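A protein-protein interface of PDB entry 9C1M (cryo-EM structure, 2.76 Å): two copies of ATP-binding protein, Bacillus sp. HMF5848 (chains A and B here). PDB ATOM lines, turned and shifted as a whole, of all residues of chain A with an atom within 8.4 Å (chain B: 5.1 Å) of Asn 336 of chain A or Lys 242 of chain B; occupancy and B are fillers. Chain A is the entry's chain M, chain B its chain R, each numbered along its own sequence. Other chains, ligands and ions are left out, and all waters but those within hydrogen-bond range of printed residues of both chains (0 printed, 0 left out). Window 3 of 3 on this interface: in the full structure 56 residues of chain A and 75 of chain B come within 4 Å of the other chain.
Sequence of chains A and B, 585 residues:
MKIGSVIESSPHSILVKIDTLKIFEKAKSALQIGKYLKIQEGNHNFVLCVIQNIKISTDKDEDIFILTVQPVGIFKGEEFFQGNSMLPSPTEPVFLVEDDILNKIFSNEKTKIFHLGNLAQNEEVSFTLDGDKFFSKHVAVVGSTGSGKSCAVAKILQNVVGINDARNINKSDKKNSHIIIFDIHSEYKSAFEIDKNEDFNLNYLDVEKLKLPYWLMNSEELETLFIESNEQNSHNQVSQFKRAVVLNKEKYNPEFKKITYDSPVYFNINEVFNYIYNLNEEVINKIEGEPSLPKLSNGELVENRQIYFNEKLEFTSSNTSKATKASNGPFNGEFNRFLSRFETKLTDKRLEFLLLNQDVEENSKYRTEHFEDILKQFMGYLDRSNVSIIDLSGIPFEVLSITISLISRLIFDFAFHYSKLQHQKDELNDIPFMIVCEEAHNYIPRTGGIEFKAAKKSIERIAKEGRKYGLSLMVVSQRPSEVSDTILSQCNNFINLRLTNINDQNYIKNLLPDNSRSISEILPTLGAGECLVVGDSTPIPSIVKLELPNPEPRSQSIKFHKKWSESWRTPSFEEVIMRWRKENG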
ATOM      1  N   GLU A 231     -15.198  -4.259 -11.390  1.00  0.00           N
ATOM      2  CA  GLU A 231     -14.589  -2.946 -11.531  1.00  0.00           C
ATOM      3  C   GLU A 231     -14.434  -2.324 -10.151  1.00  0.00           C
ATOM      4  O   GLU A 231     -15.165  -2.660  -9.217  1.00  0.00           O
ATOM      5  CB  GLU A 231     -15.415  -2.032 -12.446  1.00  0.00           C
ATOM      6  CG  GLU A 231     -14.979  -2.071 -13.904  1.00  0.00           C
ATOM      7  CD  GLU A 231     -15.743  -1.092 -14.774  1.00  0.00           C
ATOM      8  OE1 GLU A 231     -16.683  -0.448 -14.263  1.00  0.00           O
ATOM      9  OE2 GLU A 231     -15.404  -0.968 -15.970  1.00  0.00           O
ATOM     10  N   GLN A 237     -21.556   3.377  -9.981  1.00  0.00           N
ATOM     11  CA  GLN A 237     -22.522   2.925 -10.979  1.00  0.00           C
ATOM     12  C   GLN A 237     -23.791   2.390 -10.328  1.00  0.00           C
ATOM     13  O   GLN A 237     -24.896   2.662 -10.809  1.00  0.00           O
ATOM     14  CB  GLN A 237     -21.917   1.874 -11.915  1.00  0.00           C
ATOM     15  CG  GLN A 237     -20.802   2.378 -12.826  1.00  0.00           C
ATOM     16  CD  GLN A 237     -19.459   2.442 -12.154  1.00  0.00           C
ATOM     17  OE1 GLN A 237     -19.253   1.829 -11.117  1.00  0.00           O
ATOM     18  NE2 GLN A 237     -18.531   3.186 -12.744  1.00  0.00           N
ATOM     19  N   PHE A 273     -30.466   4.857 -20.155  1.00  0.00           N
ATOM     20  CA  PHE A 273     -29.222   4.814 -20.916  1.00  0.00           C
ATOM     21  C   PHE A 273     -28.792   6.210 -21.346  1.00  0.00           C
ATOM     22  O   PHE A 273     -27.611   6.564 -21.244  1.00  0.00           O
ATOM     23  CB  PHE A 273     -29.384   3.897 -22.129  1.00  0.00           C
ATOM     24  CG  PHE A 273     -28.376   4.138 -23.216  1.00  0.00           C
ATOM     25  CD1 PHE A 273     -27.039   3.833 -23.019  1.00  0.00           C
ATOM     26  CD2 PHE A 273     -28.766   4.664 -24.437  1.00  0.00           C
ATOM     27  CE1 PHE A 273     -26.109   4.052 -24.019  1.00  0.00           C
ATOM     28  CE2 PHE A 273     -27.840   4.884 -25.440  1.00  0.00           C
ATOM     29  CZ  PHE A 273     -26.511   4.578 -25.230  1.00  0.00           C
ATOM     30  N   ILE A 276     -27.428   8.051 -18.313  1.00  0.00           N
ATOM     31  CA  ILE A 276     -26.048   7.674 -18.026  1.00  0.00           C
ATOM     32  C   ILE A 276     -25.102   8.292 -19.050  1.00  0.00           C
ATOM     33  O   ILE A 276     -23.989   8.714 -18.712  1.00  0.00           O
ATOM     34  CB  ILE A 276     -25.910   6.141 -17.973  1.00  0.00           C
ATOM     35  CG1 ILE A 276     -26.818   5.562 -16.887  1.00  0.00           C
ATOM     36  CG2 ILE A 276     -24.467   5.737 -17.715  1.00  0.00           C
ATOM     37  CD1 ILE A 276     -26.825   4.049 -16.840  1.00  0.00           C
ATOM     38  N   TYR A 277     -25.527   8.358 -20.315  1.00  0.00           N
ATOM     39  CA  TYR A 277     -24.687   8.947 -21.354  1.00  0.00           C
ATOM     40  C   TYR A 277     -24.416  10.421 -21.079  1.00  0.00           C
ATOM     41  O   TYR A 277     -23.280  10.890 -21.207  1.00  0.00           O
ATOM     42  CB  TYR A 277     -25.346   8.769 -22.722  1.00  0.00           C
ATOM     43  CG  TYR A 277     -24.622   9.476 -23.846  1.00  0.00           C
ATOM     44  CD1 TYR A 277     -23.499   8.912 -24.438  1.00  0.00           C
ATOM     45  CD2 TYR A 277     -25.057  10.710 -24.313  1.00  0.00           C
ATOM     46  CE1 TYR A 277     -22.833   9.555 -25.465  1.00  0.00           C
ATOM     47  CE2 TYR A 277     -24.398  11.360 -25.337  1.00  0.00           C
ATOM     48  CZ  TYR A 277     -23.287  10.779 -25.910  1.00  0.00           C
ATOM     49  OH  TYR A 277     -22.628  11.424 -26.932  1.00  0.00           O
ATOM     50  N   ASN A 280     -21.977  11.120 -18.373  1.00  0.00           N
ATOM     51  CA  ASN A 280     -20.594  10.844 -18.743  1.00  0.00           C
ATOM     52  C   ASN A 280     -19.885  12.064 -19.316  1.00  0.00           C
ATOM     53  O   ASN A 280     -18.651  12.118 -19.281  1.00  0.00           O
ATOM     54  CB  ASN A 280     -20.546   9.696 -19.752  1.00  0.00           C
ATOM     55  CG  ASN A 280     -19.239   8.930 -19.704  1.00  0.00           C
ATOM     56  OD1 ASN A 280     -18.844   8.421 -18.655  1.00  0.00           O
ATOM     57  ND2 ASN A 280     -18.560   8.846 -20.842  1.00  0.00           N
ATOM     58  N   GLU A 281     -20.626  13.038 -19.845  1.00  0.00           N
ATOM     59  CA  GLU A 281     -20.044  14.211 -20.486  1.00  0.00           C
ATOM     60  C   GLU A 281     -20.499  15.505 -19.818  1.00  0.00           C
ATOM     61  O   GLU A 281     -20.610  16.544 -20.472  1.00  0.00           O
ATOM     62  CB  GLU A 281     -20.385  14.233 -21.976  1.00  0.00           C
ATOM     63  CG  GLU A 281     -20.139  12.915 -22.692  1.00  0.00           C
ATOM     64  CD  GLU A 281     -18.723  12.792 -23.220  1.00  0.00           C
ATOM     65  OE1 GLU A 281     -18.161  13.815 -23.664  1.00  0.00           O
ATOM     66  OE2 GLU A 281     -18.172  11.671 -23.190  1.00  0.00           O
ATOM     67  N   PHE A 331     -18.842  13.010 -12.577  1.00  0.00           N
ATOM     68  CA  PHE A 331     -19.056  11.738 -13.255  1.00  0.00           C
ATOM     69  C   PHE A 331     -18.635  11.808 -14.720  1.00  0.00           C
ATOM     70  O   PHE A 331     -19.170  11.084 -15.563  1.00  0.00           O
ATOM     71  CB  PHE A 331     -20.517  11.308 -13.140  1.00  0.00           C
ATOM     72  CG  PHE A 331     -21.036  11.298 -11.730  1.00  0.00           C
ATOM     73  CD1 PHE A 331     -20.519  10.419 -10.793  1.00  0.00           C
ATOM     74  CD2 PHE A 331     -22.039  12.171 -11.342  1.00  0.00           C
ATOM     75  CE1 PHE A 331     -20.995  10.410  -9.495  1.00  0.00           C
ATOM     76  CE2 PHE A 331     -22.519  12.166 -10.046  1.00  0.00           C
ATOM     77  CZ  PHE A 331     -21.996  11.284  -9.120  1.00  0.00           C
ATOM     78  N   ASN A 332     -17.672  12.671 -15.036  1.00  0.00           N
ATOM     79  CA  ASN A 332     -17.261  12.886 -16.418  1.00  0.00           C
ATOM     80  C   ASN A 332     -16.351  11.752 -16.875  1.00  0.00           C
ATOM     81  O   ASN A 332     -15.254  11.570 -16.335  1.00  0.00           O
ATOM     82  CB  ASN A 332     -16.554  14.232 -16.557  1.00  0.00           C
ATOM     83  CG  ASN A 332     -16.550  14.744 -17.984  1.00  0.00           C
ATOM     84  OD1 ASN A 332     -15.928  14.153 -18.866  1.00  0.00           O
ATOM     85  ND2 ASN A 332     -17.247  15.850 -18.217  1.00  0.00           N
ATOM     86  N   GLY A 333     -16.807  10.991 -17.869  1.00  0.00           N
ATOM     87  CA  GLY A 333     -15.997   9.941 -18.454  1.00  0.00           C
ATOM     88  C   GLY A 333     -15.815   8.706 -17.605  1.00  0.00           C
ATOM     89  O   GLY A 333     -14.964   7.872 -17.929  1.00  0.00           O
ATOM     90  N   GLU A 334     -16.583   8.557 -16.528  1.00  0.00           N
ATOM     91  CA  GLU A 334     -16.439   7.417 -15.634  1.00  0.00           C
ATOM     92  C   GLU A 334     -17.330   6.240 -16.007  1.00  0.00           C
ATOM     93  O   GLU A 334     -17.218   5.180 -15.383  1.00  0.00           O
ATOM     94  CB  GLU A 334     -16.739   7.840 -14.191  1.00  0.00           C
ATOM     95  CG  GLU A 334     -15.675   8.730 -13.572  1.00  0.00           C
ATOM     96  CD  GLU A 334     -16.089   9.282 -12.221  1.00  0.00           C
ATOM     97  OE1 GLU A 334     -17.177   8.908 -11.733  1.00  0.00           O
ATOM     98  OE2 GLU A 334     -15.328  10.090 -11.649  1.00  0.00           O
ATOM     99  N   PHE A 335     -18.204   6.393 -17.006  1.00  0.00           N
ATOM    100  CA  PHE A 335     -19.162   5.353 -17.367  1.00  0.00           C
ATOM    101  C   PHE A 335     -18.977   4.865 -18.801  1.00  0.00           C
ATOM    102  O   PHE A 335     -19.918   4.324 -19.388  1.00  0.00           O
ATOM    103  CB  PHE A 335     -20.595   5.854 -17.170  1.00  0.00           C
ATOM    104  CG  PHE A 335     -20.971   6.094 -15.732  1.00  0.00           C
ATOM    105  CD1 PHE A 335     -20.255   5.508 -14.702  1.00  0.00           C
ATOM    106  CD2 PHE A 335     -22.043   6.910 -15.415  1.00  0.00           C
ATOM    107  CE1 PHE A 335     -20.602   5.737 -13.383  1.00  0.00           C
ATOM    108  CE2 PHE A 335     -22.396   7.137 -14.098  1.00  0.00           C
ATOM    109  CZ  PHE A 335     -21.674   6.549 -13.081  1.00  0.00           C
ATOM    110  N   ASN A 336     -17.786   5.047 -19.380  1.00  0.00           N
ATOM    111  CA  ASN A 336     -17.581   4.688 -20.781  1.00  0.00           C
ATOM    112  C   ASN A 336     -17.759   3.190 -21.006  1.00  0.00           C
ATOM    113  O   ASN A 336     -18.528   2.768 -21.877  1.00  0.00           O
ATOM    114  CB  ASN A 336     -16.194   5.145 -21.239  1.00  0.00           C
ATOM    115  CG  ASN A 336     -15.109   4.808 -20.236  1.00  0.00           C
ATOM    116  OD1 ASN A 336     -15.391   4.342 -19.132  1.00  0.00           O
ATOM    117  ND2 ASN A 336     -13.858   5.042 -20.617  1.00  0.00           N
ATOM    118  N   ARG A 337     -17.055   2.369 -20.223  1.00  0.00           N
ATOM    119  CA  ARG A 337     -17.221   0.922 -20.332  1.00  0.00           C
ATOM    120  C   ARG A 337     -18.617   0.501 -19.893  1.00  0.00           C
ATOM    121  O   ARG A 337     -19.216  -0.409 -20.482  1.00  0.00           O
ATOM    122  CB  ARG A 337     -16.154   0.204 -19.505  1.00  0.00           C
ATOM    123  CG  ARG A 337     -14.783   0.124 -20.165  1.00  0.00           C
ATOM    124  CD  ARG A 337     -14.010   1.428 -20.028  1.00  0.00           C
ATOM    125  NE  ARG A 337     -13.788   1.794 -18.635  1.00  0.00           N
ATOM    126  CZ  ARG A 337     -12.655   1.587 -17.977  1.00  0.00           C
ATOM    127  NH1 ARG A 337     -11.612   1.018 -18.557  1.00  0.00           N
ATOM    128  NH2 ARG A 337     -12.567   1.962 -16.704  1.00  0.00           N
ATOM    129  N   PHE A 338     -19.146   1.155 -18.855  1.00  0.00           N
ATOM    130  CA  PHE A 338     -20.506   0.876 -18.412  1.00  0.00           C
ATOM    131  C   PHE A 338     -21.497   1.175 -19.531  1.00  0.00           C
ATOM    132  O   PHE A 338     -22.393   0.371 -19.806  1.00  0.00           O
ATOM    133  CB  PHE A 338     -20.811   1.709 -17.160  1.00  0.00           C
ATOM    134  CG  PHE A 338     -22.202   1.521 -16.596  1.00  0.00           C
ATOM    135  CD1 PHE A 338     -22.969   0.408 -16.906  1.00  0.00           C
ATOM    136  CD2 PHE A 338     -22.739   2.476 -15.747  1.00  0.00           C
ATOM    137  CE1 PHE A 338     -24.238   0.253 -16.380  1.00  0.00           C
ATOM    138  CE2 PHE A 338     -24.007   2.325 -15.220  1.00  0.00           C
ATOM    139  CZ  PHE A 338     -24.757   1.212 -15.537  1.00  0.00           C
ATOM    140  N   LEU A 339     -21.330   2.314 -20.210  1.00  0.00           N
ATOM    141  CA  LEU A 339     -22.215   2.658 -21.320  1.00  0.00           C
ATOM    142  C   LEU A 339     -22.073   1.672 -22.472  1.00  0.00           C
ATOM    143  O   LEU A 339     -23.066   1.311 -23.116  1.00  0.00           O
ATOM    144  CB  LEU A 339     -21.932   4.080 -21.798  1.00  0.00           C
ATOM    145  CG  LEU A 339     -22.604   5.215 -21.024  1.00  0.00           C
ATOM    146  CD1 LEU A 339     -21.956   6.544 -21.373  1.00  0.00           C
ATOM    147  CD2 LEU A 339     -24.094   5.247 -21.317  1.00  0.00           C
ATOM    148  N   SER A 340     -20.843   1.239 -22.762  1.00  0.00           N
ATOM    149  CA  SER A 340     -20.633   0.288 -23.850  1.00  0.00           C
ATOM    150  C   SER A 340     -21.341  -1.030 -23.570  1.00  0.00           C
ATOM    151  O   SER A 340     -22.052  -1.563 -24.430  1.00  0.00           O
ATOM    152  CB  SER A 340     -19.138   0.058 -24.066  1.00  0.00           C
ATOM    153  OG  SER A 340     -18.546  -0.542 -22.927  1.00  0.00           O
ATOM    154  N   ARG A 341     -21.162  -1.570 -22.361  1.00  0.00           N
ATOM    155  CA  ARG A 341     -21.840  -2.815 -22.011  1.00  0.00           C
ATOM    156  C   ARG A 341     -23.350  -2.624 -21.936  1.00  0.00           C
ATOM    157  O   ARG A 341     -24.108  -3.542 -22.274  1.00  0.00           O
ATOM    158  CB  ARG A 341     -21.301  -3.363 -20.689  1.00  0.00           C
ATOM    159  CG  ARG A 341     -19.792  -3.587 -20.664  1.00  0.00           C
ATOM    160  CD  ARG A 341     -19.267  -4.079 -22.009  1.00  0.00           C
ATOM    161  NE  ARG A 341     -17.818  -3.958 -22.110  1.00  0.00           N
ATOM    162  CZ  ARG A 341     -17.117  -4.246 -23.197  1.00  0.00           C
ATOM    163  NH1 ARG A 341     -17.700  -4.682 -24.302  1.00  0.00           N
ATOM    164  NH2 ARG A 341     -15.796  -4.091 -23.177  1.00  0.00           N
ATOM    165  N   PHE A 342     -23.801  -1.441 -21.515  1.00  0.00           N
ATOM    166  CA  PHE A 342     -25.226  -1.140 -21.494  1.00  0.00           C
ATOM    167  C   PHE A 342     -25.816  -1.212 -22.895  1.00  0.00           C
ATOM    168  O   PHE A 342     -26.839  -1.868 -23.122  1.00  0.00           O
ATOM    169  CB  PHE A 342     -25.436   0.247 -20.884  1.00  0.00           C
ATOM    170  CG  PHE A 342     -26.715   0.393 -20.121  1.00  0.00           C
ATOM    171  CD1 PHE A 342     -27.866   0.835 -20.746  1.00  0.00           C
ATOM    172  CD2 PHE A 342     -26.763   0.095 -18.772  1.00  0.00           C
ATOM    173  CE1 PHE A 342     -29.043   0.973 -20.040  1.00  0.00           C
ATOM    174  CE2 PHE A 342     -27.934   0.230 -18.064  1.00  0.00           C
ATOM    175  CZ  PHE A 342     -29.076   0.670 -18.695  1.00  0.00           C
ATOM    176  N   GLU A 343     -25.164  -0.554 -23.855  1.00  0.00           N
ATOM    177  CA  GLU A 343     -25.638  -0.590 -25.234  1.00  0.00           C
ATOM    178  C   GLU A 343     -25.563  -2.001 -25.805  1.00  0.00           C
ATOM    179  O   GLU A 343     -26.457  -2.427 -26.545  1.00  0.00           O
ATOM    180  CB  GLU A 343     -24.832   0.382 -26.097  1.00  0.00           C
ATOM    181  CG  GLU A 343     -25.539   0.796 -27.378  1.00  0.00           C
ATOM    182  CD  GLU A 343     -24.671   1.660 -28.271  1.00  0.00           C
ATOM    183  OE1 GLU A 343     -23.657   1.148 -28.791  1.00  0.00           O
ATOM    184  OE2 GLU A 343     -25.003   2.850 -28.454  1.00  0.00           O
ATOM    185  N   THR A 344     -24.502  -2.743 -25.469  1.00  0.00           N
ATOM    186  CA  THR A 344     -24.385  -4.119 -25.942  1.00  0.00           C
ATOM    187  C   THR A 344     -25.541  -4.974 -25.438  1.00  0.00           C
ATOM    188  O   THR A 344     -26.108  -5.773 -26.192  1.00  0.00           O
ATOM    189  CB  THR A 344     -23.047  -4.714 -25.502  1.00  0.00           C
ATOM    190  OG1 THR A 344     -21.975  -3.937 -26.051  1.00  0.00           O
ATOM    191  CG2 THR A 344     -22.918  -6.153 -25.978  1.00  0.00           C
ATOM    192  N   GLU B 223     -11.575  -3.044 -28.267  1.00  0.00           N
ATOM    193  CA  GLU B 223     -10.919  -2.216 -27.263  1.00  0.00           C
ATOM    194  C   GLU B 223      -9.643  -2.873 -26.754  1.00  0.00           C
ATOM    195  O   GLU B 223      -8.612  -2.209 -26.611  1.00  0.00           O
ATOM    196  CB  GLU B 223     -11.882  -1.934 -26.109  1.00  0.00           C
ATOM    197  CG  GLU B 223     -12.992  -0.954 -26.457  1.00  0.00           C
ATOM    198  CD  GLU B 223     -13.917  -0.678 -25.287  1.00  0.00           C
ATOM    199  OE1 GLU B 223     -13.584  -1.087 -24.155  1.00  0.00           O
ATOM    200  OE2 GLU B 223     -14.977  -0.053 -25.501  1.00  0.00           O
ATOM    201  N   VAL B 238     -10.770   6.337 -25.045  1.00  0.00           N
ATOM    202  CA  VAL B 238     -11.637   5.233 -25.447  1.00  0.00           C
ATOM    203  C   VAL B 238     -12.869   5.761 -26.174  1.00  0.00           C
ATOM    204  O   VAL B 238     -13.261   5.243 -27.226  1.00  0.00           O
ATOM    205  CB  VAL B 238     -12.023   4.386 -24.222  1.00  0.00           C
ATOM    206  CG1 VAL B 238     -12.788   3.145 -24.646  1.00  0.00           C
ATOM    207  CG2 VAL B 238     -10.781   4.008 -23.429  1.00  0.00           C
ATOM    208  N   SER B 239     -13.490   6.809 -25.625  1.00  0.00           N
ATOM    209  CA  SER B 239     -14.725   7.330 -26.203  1.00  0.00           C
ATOM    210  C   SER B 239     -14.501   7.854 -27.615  1.00  0.00           C
ATOM    211  O   SER B 239     -15.325   7.625 -28.508  1.00  0.00           O
ATOM    212  CB  SER B 239     -15.298   8.428 -25.307  1.00  0.00           C
ATOM    213  OG  SER B 239     -16.311   9.158 -25.979  1.00  0.00           O
ATOM    214  N   GLN B 240     -13.393   8.568 -27.834  1.00  0.00           N
ATOM    215  CA  GLN B 240     -13.088   9.057 -29.174  1.00  0.00           C
ATOM    216  C   GLN B 240     -12.865   7.904 -30.143  1.00  0.00           C
ATOM    217  O   GLN B 240     -13.290   7.969 -31.301  1.00  0.00           O
ATOM    218  CB  GLN B 240     -11.867   9.975 -29.139  1.00  0.00           C
ATOM    219  CG  GLN B 240     -12.166  11.377 -28.637  1.00  0.00           C
ATOM    220  CD  GLN B 240     -13.365  11.993 -29.328  1.00  0.00           C
ATOM    221  OE1 GLN B 240     -14.418  12.185 -28.719  1.00  0.00           O
ATOM    222  NE2 GLN B 240     -13.212  12.312 -30.609  1.00  0.00           N
ATOM    223  N   PHE B 241     -12.199   6.840 -29.689  1.00  0.00           N
ATOM    224  CA  PHE B 241     -11.988   5.678 -30.546  1.00  0.00           C
ATOM    225  C   PHE B 241     -13.314   5.035 -30.935  1.00  0.00           C
ATOM    226  O   PHE B 241     -13.535   4.694 -32.104  1.00  0.00           O
ATOM    227  CB  PHE B 241     -11.091   4.663 -29.839  1.00  0.00           C
ATOM    228  CG  PHE B 241     -10.786   3.449 -30.664  1.00  0.00           C
ATOM    229  CD1 PHE B 241      -9.870   3.513 -31.699  1.00  0.00           C
ATOM    230  CD2 PHE B 241     -11.432   2.249 -30.420  1.00  0.00           C
ATOM    231  CE1 PHE B 241      -9.589   2.398 -32.462  1.00  0.00           C
ATOM    232  CE2 PHE B 241     -11.156   1.132 -31.181  1.00  0.00           C
ATOM    233  CZ  PHE B 241     -10.236   1.207 -32.203  1.00  0.00           C
ATOM    234  N   LYS B 242     -14.213   4.863 -29.961  1.00  0.00           N
ATOM    235  CA  LYS B 242     -15.518   4.276 -30.249  1.00  0.00           C
ATOM    236  C   LYS B 242     -16.312   5.147 -31.214  1.00  0.00           C
ATOM    237  O   LYS B 242     -16.942   4.639 -32.152  1.00  0.00           O
ATOM    238  CB  LYS B 242     -16.296   4.079 -28.949  1.00  0.00           C
ATOM    239  CG  LYS B 242     -15.533   3.321 -27.881  1.00  0.00           C
ATOM    240  CD  LYS B 242     -16.454   2.571 -26.939  1.00  0.00           C
ATOM    241  CE  LYS B 242     -16.291   3.098 -25.524  1.00  0.00           C
ATOM    242  NZ  LYS B 242     -16.756   2.136 -24.494  1.00  0.00           N
ATOM    243  N   ARG B 243     -16.296   6.464 -30.993  1.00  0.00           N
ATOM    244  CA  ARG B 243     -17.019   7.376 -31.872  1.00  0.00           C
ATOM    245  C   ARG B 243     -16.453   7.336 -33.286  1.00  0.00           C
ATOM    246  O   ARG B 243     -17.208   7.327 -34.265  1.00  0.00           O
ATOM    247  CB  ARG B 243     -16.966   8.794 -31.304  1.00  0.00           C
ATOM    248  CG  ARG B 243     -17.968   9.756 -31.918  1.00  0.00           C
ATOM    249  CD  ARG B 243     -17.952  11.089 -31.186  1.00  0.00           C
ATOM    250  NE  ARG B 243     -19.009  11.173 -30.186  1.00  0.00           N
ATOM    251  CZ  ARG B 243     -18.796  11.294 -28.881  1.00  0.00           C
ATOM    252  NH1 ARG B 243     -17.572  11.349 -28.383  1.00  0.00           N
ATOM    253  NH2 ARG B 243     -19.839  11.362 -28.058  1.00  0.00           N
ATOM    254  N   ALA B 244     -15.125   7.302 -33.411  1.00  0.00           N
ATOM    255  CA  ALA B 244     -14.503   7.200 -34.725  1.00  0.00           C
ATOM    256  C   ALA B 244     -14.899   5.909 -35.423  1.00  0.00           C
ATOM    257  O   ALA B 244     -15.222   5.914 -36.617  1.00  0.00           O
ATOM    258  CB  ALA B 244     -12.985   7.281 -34.591  1.00  0.00           C
ATOM    259  N   VAL B 245     -14.878   4.791 -34.695  1.00  0.00           N
ATOM    260  CA  VAL B 245     -15.204   3.507 -35.304  1.00  0.00           C
ATOM    261  C   VAL B 245     -16.652   3.491 -35.777  1.00  0.00           C
ATOM    262  O   VAL B 245     -16.945   3.061 -36.899  1.00  0.00           O
ATOM    263  CB  VAL B 245     -14.910   2.357 -34.323  1.00  0.00           C
ATOM    264  CG1 VAL B 245     -15.515   1.058 -34.830  1.00  0.00           C
ATOM    265  CG2 VAL B 245     -13.411   2.201 -34.129  1.00  0.00           C
ATOM    266  N   VAL B 246     -17.579   3.974 -34.944  1.00  0.00           N
ATOM    267  CA  VAL B 246     -18.986   3.935 -35.336  1.00  0.00           C
ATOM    268  C   VAL B 246     -19.252   4.903 -36.486  1.00  0.00           C
ATOM    269  O   VAL B 246     -20.038   4.603 -37.393  1.00  0.00           O
ATOM    270  CB  VAL B 246     -19.907   4.209 -34.129  1.00  0.00           C
ATOM    271  CG1 VAL B 246     -19.722   3.138 -33.069  1.00  0.00           C
ATOM    272  CG2 VAL B 246     -19.679   5.591 -33.548  1.00  0.00           C
ATOM    273  N   LEU B 247     -18.599   6.071 -36.479  1.00  0.00           N
ATOM    274  CA  LEU B 247     -18.784   7.021 -37.570  1.00  0.00           C
ATOM    275  C   LEU B 247     -18.241   6.471 -38.882  1.00  0.00           C
ATOM    276  O   LEU B 247     -18.872   6.631 -39.932  1.00  0.00           O
ATOM    277  CB  LEU B 247     -18.116   8.352 -37.227  1.00  0.00           C
ATOM    278  CG  LEU B 247     -18.973   9.343 -36.438  1.00  0.00           C
ATOM    279  CD1 LEU B 247     -18.193  10.614 -36.143  1.00  0.00           C
ATOM    280  CD2 LEU B 247     -20.257   9.659 -37.190  1.00  0.00           C
ATOM    281  N   TYR B 261     -21.731   0.216 -32.025  1.00  0.00           N
ATOM    282  CA  TYR B 261     -20.336  -0.161 -31.837  1.00  0.00           C
ATOM    283  C   TYR B 261     -20.111  -1.663 -31.947  1.00  0.00           C
ATOM    284  O   TYR B 261     -18.956  -2.095 -32.027  1.00  0.00           O
ATOM    285  CB  TYR B 261     -19.846   0.345 -30.477  1.00  0.00           C
ATOM    286  CG  TYR B 261     -18.347   0.273 -30.284  1.00  0.00           C
ATOM    287  CD1 TYR B 261     -17.476   0.689 -31.282  1.00  0.00           C
ATOM    288  CD2 TYR B 261     -17.805  -0.204 -29.100  1.00  0.00           C
ATOM    289  CE1 TYR B 261     -16.105   0.624 -31.105  1.00  0.00           C
ATOM    290  CE2 TYR B 261     -16.438  -0.275 -28.915  1.00  0.00           C
ATOM    291  CZ  TYR B 261     -15.593   0.142 -29.918  1.00  0.00           C
ATOM    292  OH  TYR B 261     -14.231   0.075 -29.734  1.00  0.00           O
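NE of Arg 337 of chain A sits at hydrogen-bond distance from OD1 of Asn 336 of chain A, 3.1 Å away. OE1 of Gln 240 of chain B lies within hydrogen-bond range of NH1 of Arg 243 of chain B, 3.3 Å away. The guanidinium group of Arg 243 of chain B sits at hydrogen-bond distance from the side-chain hydroxyl of Ser 239 of chain B. The side-chain carboxylate of Glu 223 of chain B is in salt-bridge range of the side-chain amino group of Lys 242 of chain B (3.0 Å). OG1 of Thr 344 of chain A is in hydrogen-bond range of O of Ser 340 of chain A, 2.9 Å away. O of Arg 337 of chain A lies within hydrogen-bond range of OG of Ser 340 of chain A, at 2.5 Å.
Hydrophobic or aromatic side chains of chain A within 4 Å of the printed part of chain B: Tyr 277. Among the printed residues, 5 pairs touch across the chains.
Asn 336 of chain A touches just one residue of chain B: Lys 242. Of the printed residues of chain B, Ser 340 of chain A touches Lys 242 (3.2 Å). Printed residues of chain B within 4 Å of Glu 343 of chain A: Tyr 261. Of the printed residues of chain A, Glu 223 of chain B touches Arg 341 (3.9 Å). Ser 239 of chain B touches none of the printed residues of chain A. Lys 242 of chain B touches just these residues of chain A: Asn 336 (3.2 Å) and Ser 340 (3.2 Å). Printed residues of chain A within 4 Å of Tyr 261 of chain B: Glu 343 (3.9 Å). The nearest residue of chain B that does not touch Asn 336 of chain A is Val 238 of chain B (4.1 Å). The nearest residue of chain A that does not touch Lys 242 of chain B is Arg 337 of chain A (4.3 Å). The nearest printed residue of chain B that does not touch Glu 343 of chain A is Val 246 of chain B (6.1 Å).
No position is printed for both chains. Of the 5 pairs that touch across the chains among the printed residues, none has its exchanged pair printed and touching as well.
Among the printed residues, pairs that only touch across the chains: Ser 340 of chain A with Lys 242 of chain B and Glu 343 of chain A with Tyr 261 of chain B.
The side-chain hydroxyl of Tyr 277 of chain A is in hydrogen-bond range of the guanidinium group of Arg 243 of chain B, at 3.0 Å. NH2 of Arg 341 of chain A is in salt-bridge range of OE1 of Glu 223 of chain B. The side-chain amino group (NZ) of Lys 242 of chain B sits at hydrogen-bond distance from the backbone carbonyl oxygen (O) of Asn 336 of chain A, 3.2 Å away.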
